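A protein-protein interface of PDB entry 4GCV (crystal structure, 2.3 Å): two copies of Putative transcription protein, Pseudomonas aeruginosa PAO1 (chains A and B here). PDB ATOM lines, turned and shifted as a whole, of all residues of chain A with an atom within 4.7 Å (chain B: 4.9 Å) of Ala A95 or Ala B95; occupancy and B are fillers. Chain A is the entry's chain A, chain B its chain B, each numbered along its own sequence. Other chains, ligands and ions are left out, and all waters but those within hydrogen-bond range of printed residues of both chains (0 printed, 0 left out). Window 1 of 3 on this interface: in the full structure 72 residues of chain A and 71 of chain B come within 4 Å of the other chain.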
ATOM      1  N   VAL A  91     -22.904 -13.193  17.338  1.00  0.00           N
ATOM      2  CA  VAL A  91     -23.396 -14.484  17.781  1.00  0.00           C
ATOM      3  C   VAL A  91     -24.867 -14.609  17.473  1.00  0.00           C
ATOM      4  O   VAL A  91     -25.340 -15.702  17.180  1.00  0.00           O
ATOM      5  CB  VAL A  91     -23.186 -14.625  19.285  1.00  0.00           C
ATOM      6  CG1 VAL A  91     -23.768 -15.930  19.858  1.00  0.00           C
ATOM      7  CG2 VAL A  91     -21.695 -14.542  19.558  1.00  0.00           C
ATOM      8  N   VAL A  92     -25.584 -13.493  17.558  1.00  0.00           N
ATOM      9  CA  VAL A  92     -26.983 -13.468  17.233  1.00  0.00           C
ATOM     10  C   VAL A  92     -27.145 -13.653  15.712  1.00  0.00           C
ATOM     11  O   VAL A  92     -27.982 -14.419  15.285  1.00  0.00           O
ATOM     12  CB  VAL A  92     -27.619 -12.134  17.723  1.00  0.00           C
ATOM     13  CG1 VAL A  92     -29.002 -11.907  17.111  1.00  0.00           C
ATOM     14  CG2 VAL A  92     -27.611 -12.041  19.258  1.00  0.00           C
ATOM     15  N   LEU A  93     -26.360 -12.942  14.894  1.00  0.00           N
ATOM     16  CA  LEU A  93     -26.472 -13.118  13.440  1.00  0.00           C
ATOM     17  C   LEU A  93     -26.229 -14.562  13.077  1.00  0.00           C
ATOM     18  O   LEU A  93     -27.004 -15.136  12.302  1.00  0.00           O
ATOM     19  CB  LEU A  93     -25.524 -12.252  12.609  1.00  0.00           C
ATOM     20  CG  LEU A  93     -25.483 -10.730  12.780  1.00  0.00           C
ATOM     21  CD1 LEU A  93     -24.352 -10.191  11.877  1.00  0.00           C
ATOM     22  CD2 LEU A  93     -26.847  -9.979  12.574  1.00  0.00           C
ATOM     23  N   MET A  94     -25.176 -15.143  13.632  1.00  0.00           N
ATOM     24  CA  MET A  94     -24.863 -16.538  13.354  1.00  0.00           C
ATOM     25  C   MET A  94     -25.935 -17.492  13.874  1.00  0.00           C
ATOM     26  O   MET A  94     -26.258 -18.494  13.211  1.00  0.00           O
ATOM     27  CB  MET A  94     -23.521 -16.897  13.928  1.00  0.00           C
ATOM     28  CG  MET A  94     -22.421 -16.175  13.238  1.00  0.00           C
ATOM     29  SD  MET A  94     -20.670 -16.617  13.938  1.00  0.00           S
ATOM     30  CE  MET A  94     -19.720 -16.302  12.297  1.00  0.00           C
ATOM     31  N   ALA A  95     -26.503 -17.186  15.038  1.00  0.00           N
ATOM     32  CA  ALA A  95     -27.574 -18.030  15.536  1.00  0.00           C
ATOM     33  C   ALA A  95     -28.789 -17.993  14.584  1.00  0.00           C
ATOM     34  O   ALA A  95     -29.426 -19.049  14.361  1.00  0.00           O
ATOM     35  CB  ALA A  95     -27.983 -17.681  16.985  1.00  0.00           C
ATOM     36  N   PHE A  96     -29.112 -16.814  14.036  1.00  0.00           N
ATOM     37  CA  PHE A  96     -30.245 -16.706  13.098  1.00  0.00           C
ATOM     38  C   PHE A  96     -29.974 -17.473  11.824  1.00  0.00           C
ATOM     39  O   PHE A  96     -30.889 -18.098  11.304  1.00  0.00           O
ATOM     40  CB  PHE A  96     -30.542 -15.283  12.674  1.00  0.00           C
ATOM     41  CG  PHE A  96     -31.512 -14.570  13.539  1.00  0.00           C
ATOM     42  CD1 PHE A  96     -32.841 -14.905  13.521  1.00  0.00           C
ATOM     43  CD2 PHE A  96     -31.078 -13.523  14.361  1.00  0.00           C
ATOM     44  CE1 PHE A  96     -33.787 -14.191  14.291  1.00  0.00           C
ATOM     45  CE2 PHE A  96     -31.988 -12.820  15.151  1.00  0.00           C
ATOM     46  CZ  PHE A  96     -33.362 -13.157  15.108  1.00  0.00           C
ATOM     47  N   VAL A  97     -28.743 -17.406  11.307  1.00  0.00           N
ATOM     48  CA  VAL A  97     -28.440 -18.251  10.211  1.00  0.00           C
ATOM     49  C   VAL A  97     -28.512 -19.748  10.482  1.00  0.00           C
ATOM     50  O   VAL A  97     -29.080 -20.454   9.656  1.00  0.00           O
ATOM     51  CB  VAL A  97     -27.283 -17.797   9.257  1.00  0.00           C
ATOM     52  CG1 VAL A  97     -26.549 -16.588   9.689  1.00  0.00           C
ATOM     53  CG2 VAL A  97     -26.395 -18.934   8.807  1.00  0.00           C
ATOM     54  N   ALA A  98     -27.995 -20.229  11.609  1.00  0.00           N
ATOM     55  CA  ALA A  98     -28.103 -21.636  11.964  1.00  0.00           C
ATOM     56  C   ALA A  98     -29.565 -22.003  12.040  1.00  0.00           C
ATOM     57  O   ALA A  98     -29.979 -23.014  11.476  1.00  0.00           O
ATOM     58  CB  ALA A  98     -27.383 -21.947  13.318  1.00  0.00           C
ATOM     59  N   TRP A  99     -30.361 -21.140  12.684  1.00  0.00           N
ATOM     60  CA  TRP A  99     -31.794 -21.328  12.776  1.00  0.00           C
ATOM     61  C   TRP A  99     -32.427 -21.461  11.403  1.00  0.00           C
ATOM     62  O   TRP A  99     -33.346 -22.284  11.184  1.00  0.00           O
ATOM     63  CB  TRP A  99     -32.394 -20.142  13.540  1.00  0.00           C
ATOM     64  CG  TRP A  99     -33.865 -20.107  13.502  1.00  0.00           C
ATOM     65  CD1 TRP A  99     -34.704 -20.865  14.232  1.00  0.00           C
ATOM     66  CD2 TRP A  99     -34.692 -19.287  12.655  1.00  0.00           C
ATOM     67  NE1 TRP A  99     -36.034 -20.605  13.879  1.00  0.00           N
ATOM     68  CE2 TRP A  99     -36.044 -19.614  12.935  1.00  0.00           C
ATOM     69  CE3 TRP A  99     -34.420 -18.294  11.700  1.00  0.00           C
ATOM     70  CZ2 TRP A  99     -37.116 -18.998  12.297  1.00  0.00           C
ATOM     71  CZ3 TRP A  99     -35.472 -17.699  11.062  1.00  0.00           C
ATOM     72  CH2 TRP A  99     -36.822 -18.055  11.360  1.00  0.00           C
ATOM     73  N   PHE A 125     -24.395 -25.394  17.754  1.00  0.00           N
ATOM     74  CA  PHE A 125     -23.746 -24.629  18.792  1.00  0.00           C
ATOM     75  C   PHE A 125     -23.629 -25.475  20.044  1.00  0.00           C
ATOM     76  O   PHE A 125     -24.477 -26.286  20.313  1.00  0.00           O
ATOM     77  CB  PHE A 125     -24.536 -23.365  19.100  1.00  0.00           C
ATOM     78  CG  PHE A 125     -24.669 -22.443  17.922  1.00  0.00           C
ATOM     79  CD1 PHE A 125     -23.548 -22.046  17.209  1.00  0.00           C
ATOM     80  CD2 PHE A 125     -25.912 -21.977  17.526  1.00  0.00           C
ATOM     81  CE1 PHE A 125     -23.662 -21.225  16.127  1.00  0.00           C
ATOM     82  CE2 PHE A 125     -26.034 -21.161  16.457  1.00  0.00           C
ATOM     83  CZ  PHE A 125     -24.892 -20.768  15.751  1.00  0.00           C
ATOM     84  N   VAL B  91     -32.543 -21.473  20.091  1.00  0.00           N
ATOM     85  CA  VAL B  91     -31.145 -21.132  19.958  1.00  0.00           C
ATOM     86  C   VAL B  91     -30.929 -19.627  19.827  1.00  0.00           C
ATOM     87  O   VAL B  91     -29.943 -19.098  20.321  1.00  0.00           O
ATOM     88  CB  VAL B  91     -30.462 -21.871  18.764  1.00  0.00           C
ATOM     89  CG1 VAL B  91     -28.945 -21.596  18.797  1.00  0.00           C
ATOM     90  CG2 VAL B  91     -30.752 -23.400  18.853  1.00  0.00           C
ATOM     91  N   VAL B  92     -31.820 -18.967  19.104  1.00  0.00           N
ATOM     92  CA  VAL B  92     -31.701 -17.557  18.848  1.00  0.00           C
ATOM     93  C   VAL B  92     -31.972 -16.780  20.154  1.00  0.00           C
ATOM     94  O   VAL B  92     -31.221 -15.908  20.495  1.00  0.00           O
ATOM     95  CB  VAL B  92     -32.647 -17.132  17.699  1.00  0.00           C
ATOM     96  CG1 VAL B  92     -32.804 -15.611  17.621  1.00  0.00           C
ATOM     97  CG2 VAL B  92     -32.142 -17.650  16.389  1.00  0.00           C
ATOM     98  N   LEU B  93     -33.030 -17.134  20.875  1.00  0.00           N
ATOM     99  CA  LEU B  93     -33.364 -16.523  22.163  1.00  0.00           C
ATOM    100  C   LEU B  93     -32.180 -16.625  23.127  1.00  0.00           C
ATOM    101  O   LEU B  93     -31.887 -15.673  23.846  1.00  0.00           O
ATOM    102  CB  LEU B  93     -34.533 -17.227  22.840  1.00  0.00           C
ATOM    103  CG  LEU B  93     -35.787 -17.498  22.010  1.00  0.00           C
ATOM    104  CD1 LEU B  93     -36.720 -18.316  22.876  1.00  0.00           C
ATOM    105  CD2 LEU B  93     -36.448 -16.183  21.509  1.00  0.00           C
ATOM    106  N   MET B  94     -31.554 -17.793  23.151  1.00  0.00           N
ATOM    107  CA  MET B  94     -30.441 -18.083  24.050  1.00  0.00           C
ATOM    108  C   MET B  94     -29.271 -17.208  23.656  1.00  0.00           C
ATOM    109  O   MET B  94     -28.520 -16.694  24.503  1.00  0.00           O
ATOM    110  CB  MET B  94     -30.069 -19.569  23.942  1.00  0.00           C
ATOM    111  CG  MET B  94     -30.711 -20.340  25.041  1.00  0.00           C
ATOM    112  SD  MET B  94     -30.422 -22.297  25.036  1.00  0.00           S
ATOM    113  CE  MET B  94     -31.203 -22.495  26.772  1.00  0.00           C
ATOM    114  N   ALA B  95     -29.121 -17.046  22.349  1.00  0.00           N
ATOM    115  CA  ALA B  95     -28.097 -16.183  21.850  1.00  0.00           C
ATOM    116  C   ALA B  95     -28.369 -14.739  22.259  1.00  0.00           C
ATOM    117  O   ALA B  95     -27.428 -14.074  22.612  1.00  0.00           O
ATOM    118  CB  ALA B  95     -27.951 -16.310  20.337  1.00  0.00           C
ATOM    119  N   PHE B  96     -29.620 -14.247  22.184  1.00  0.00           N
ATOM    120  CA  PHE B  96     -29.867 -12.855  22.548  1.00  0.00           C
ATOM    121  C   PHE B  96     -29.464 -12.658  23.992  1.00  0.00           C
ATOM    122  O   PHE B  96     -28.954 -11.596  24.339  1.00  0.00           O
ATOM    123  CB  PHE B  96     -31.338 -12.440  22.397  1.00  0.00           C
ATOM    124  CG  PHE B  96     -31.682 -11.886  21.016  1.00  0.00           C
ATOM    125  CD1 PHE B  96     -31.388 -10.575  20.689  1.00  0.00           C
ATOM    126  CD2 PHE B  96     -32.265 -12.705  20.037  1.00  0.00           C
ATOM    127  CE1 PHE B  96     -31.692 -10.071  19.408  1.00  0.00           C
ATOM    128  CE2 PHE B  96     -32.545 -12.193  18.762  1.00  0.00           C
ATOM    129  CZ  PHE B  96     -32.275 -10.890  18.464  1.00  0.00           C
ATOM    130  N   VAL B  97     -29.702 -13.662  24.850  1.00  0.00           N
ATOM    131  CA  VAL B  97     -29.276 -13.458  26.200  1.00  0.00           C
ATOM    132  C   VAL B  97     -27.769 -13.449  26.450  1.00  0.00           C
ATOM    133  O   VAL B  97     -27.321 -12.627  27.206  1.00  0.00           O
ATOM    134  CB  VAL B  97     -30.149 -14.134  27.316  1.00  0.00           C
ATOM    135  CG1 VAL B  97     -31.495 -14.702  26.845  1.00  0.00           C
ATOM    136  CG2 VAL B  97     -29.383 -14.928  28.300  1.00  0.00           C
ATOM    137  N   ALA B  98     -27.018 -14.303  25.741  1.00  0.00           N
ATOM    138  CA  ALA B  98     -25.590 -14.366  25.819  1.00  0.00           C
ATOM    139  C   ALA B  98     -25.057 -13.014  25.319  1.00  0.00           C
ATOM    140  O   ALA B  98     -24.150 -12.437  25.931  1.00  0.00           O
ATOM    141  CB  ALA B  98     -25.010 -15.554  24.985  1.00  0.00           C
ATOM    142  N   TRP B  99     -25.648 -12.510  24.243  1.00  0.00           N
ATOM    143  CA  TRP B  99     -25.372 -11.167  23.756  1.00  0.00           C
ATOM    144  C   TRP B  99     -25.595 -10.056  24.803  1.00  0.00           C
ATOM    145  O   TRP B  99     -24.707  -9.239  24.997  1.00  0.00           O
ATOM    146  CB  TRP B  99     -26.214 -10.852  22.537  1.00  0.00           C
ATOM    147  CG  TRP B  99     -26.044  -9.461  22.085  1.00  0.00           C
ATOM    148  CD1 TRP B  99     -24.985  -8.943  21.387  1.00  0.00           C
ATOM    149  CD2 TRP B  99     -26.952  -8.385  22.308  1.00  0.00           C
ATOM    150  NE1 TRP B  99     -25.194  -7.589  21.158  1.00  0.00           N
ATOM    151  CE2 TRP B  99     -26.400  -7.233  21.713  1.00  0.00           C
ATOM    152  CE3 TRP B  99     -28.213  -8.287  22.932  1.00  0.00           C
ATOM    153  CZ2 TRP B  99     -27.054  -5.995  21.727  1.00  0.00           C
ATOM    154  CZ3 TRP B  99     -28.847  -7.046  22.948  1.00  0.00           C
ATOM    155  CH2 TRP B  99     -28.262  -5.924  22.351  1.00  0.00           C
ATOM    156  N   PHE B 125     -20.918 -19.335  23.670  1.00  0.00           N
ATOM    157  CA  PHE B 125     -21.357 -20.235  22.628  1.00  0.00           C
ATOM    158  C   PHE B 125     -20.117 -20.795  21.994  1.00  0.00           C
ATOM    159  O   PHE B 125     -19.109 -20.103  21.943  1.00  0.00           O
ATOM    160  CB  PHE B 125     -22.092 -19.457  21.559  1.00  0.00           C
ATOM    161  CG  PHE B 125     -23.569 -19.401  21.751  1.00  0.00           C
ATOM    162  CD1 PHE B 125     -24.106 -19.072  22.980  1.00  0.00           C
ATOM    163  CD2 PHE B 125     -24.428 -19.681  20.666  1.00  0.00           C
ATOM    164  CE1 PHE B 125     -25.477 -19.003  23.159  1.00  0.00           C
ATOM    165  CE2 PHE B 125     -25.821 -19.604  20.815  1.00  0.00           C
ATOM    166  CZ  PHE B 125     -26.347 -19.278  22.080  1.00  0.00           C
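Of the 10 printed residues of chain A, 6 touch a printed residue of chain B. Along chain A the printed residues that touch a printed residue of chain B span positions 91 to 125. Printed residues of chain B that touch a printed residue of chain A: Val B91, Val B92, Ala B95, Phe B96, Trp B99 and Phe B125. Hydrophobic or aromatic side chains of chain B within 4 Å of the printed part of chain A: Val B91, Val B92, Ala B95, Phe B96, Trp B99 and Phe B125. Among the printed residues, 11 pairs touch across the chains.
Printed residues of chain B within 4 Å of Val A92: Ala B95 (3.9 Å), Phe B96 (3.7 Å) and Trp B99 (3.8 Å). Ala A95 touches just these residues of chain B: Val B92 and Ala B95. Of the printed residues of chain B, Phe A96 touches Val B92 and Phe B96. Of the printed residues of chain A, Val B92 touches Ala A95 (3.7 Å), Phe A96 (3.6 Å) and Trp A99 (3.8 Å). Of chain A, only Val A92 and Ala A95 come within 4 Å of Ala B95. The nearest residue of chain B that does not touch Ala A95 is Val B91 (4.1 Å). The nearest residue of chain A that does not touch Ala B95 is Val A91 (4.1 Å). The nearest printed residue of chain B that does not touch Val A92 is Val B92 (5.3 Å).
Among the printed residues, pairs that only touch across the chains: Val A91 with Phe B125 (3.9 Å), Val A92 with Ala B95 (3.9 Å), Val A92 with Phe B96 (3.7 Å), Val A92 with Trp B99 (3.8 Å), Ala A95 with Val B92 (3.7 Å), Ala A95 with Ala B95 (3.6 Å), Phe A96 with Val B92 (3.6 Å), Phe A96 with Phe B96 (3.7 Å), Trp A99 with Val B92 (3.8 Å), Phe A125 with Val B91 (3.3 Å) and Phe A125 with Phe B125 (3.9 Å).
Val A91 touches Phe B125, and with the chains exchanged Phe A125 touches Val B91. Val A92 touches Phe B96, and with the chains exchanged Phe A96 touches Val B92. Ala B95 touches its own counterpart, Ala A95. Phe B125 touches its own counterpart, Phe A125. Of the 11 pairs that touch across the chains among the printed residues, 11 have their exchanged pair printed and touching as well.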
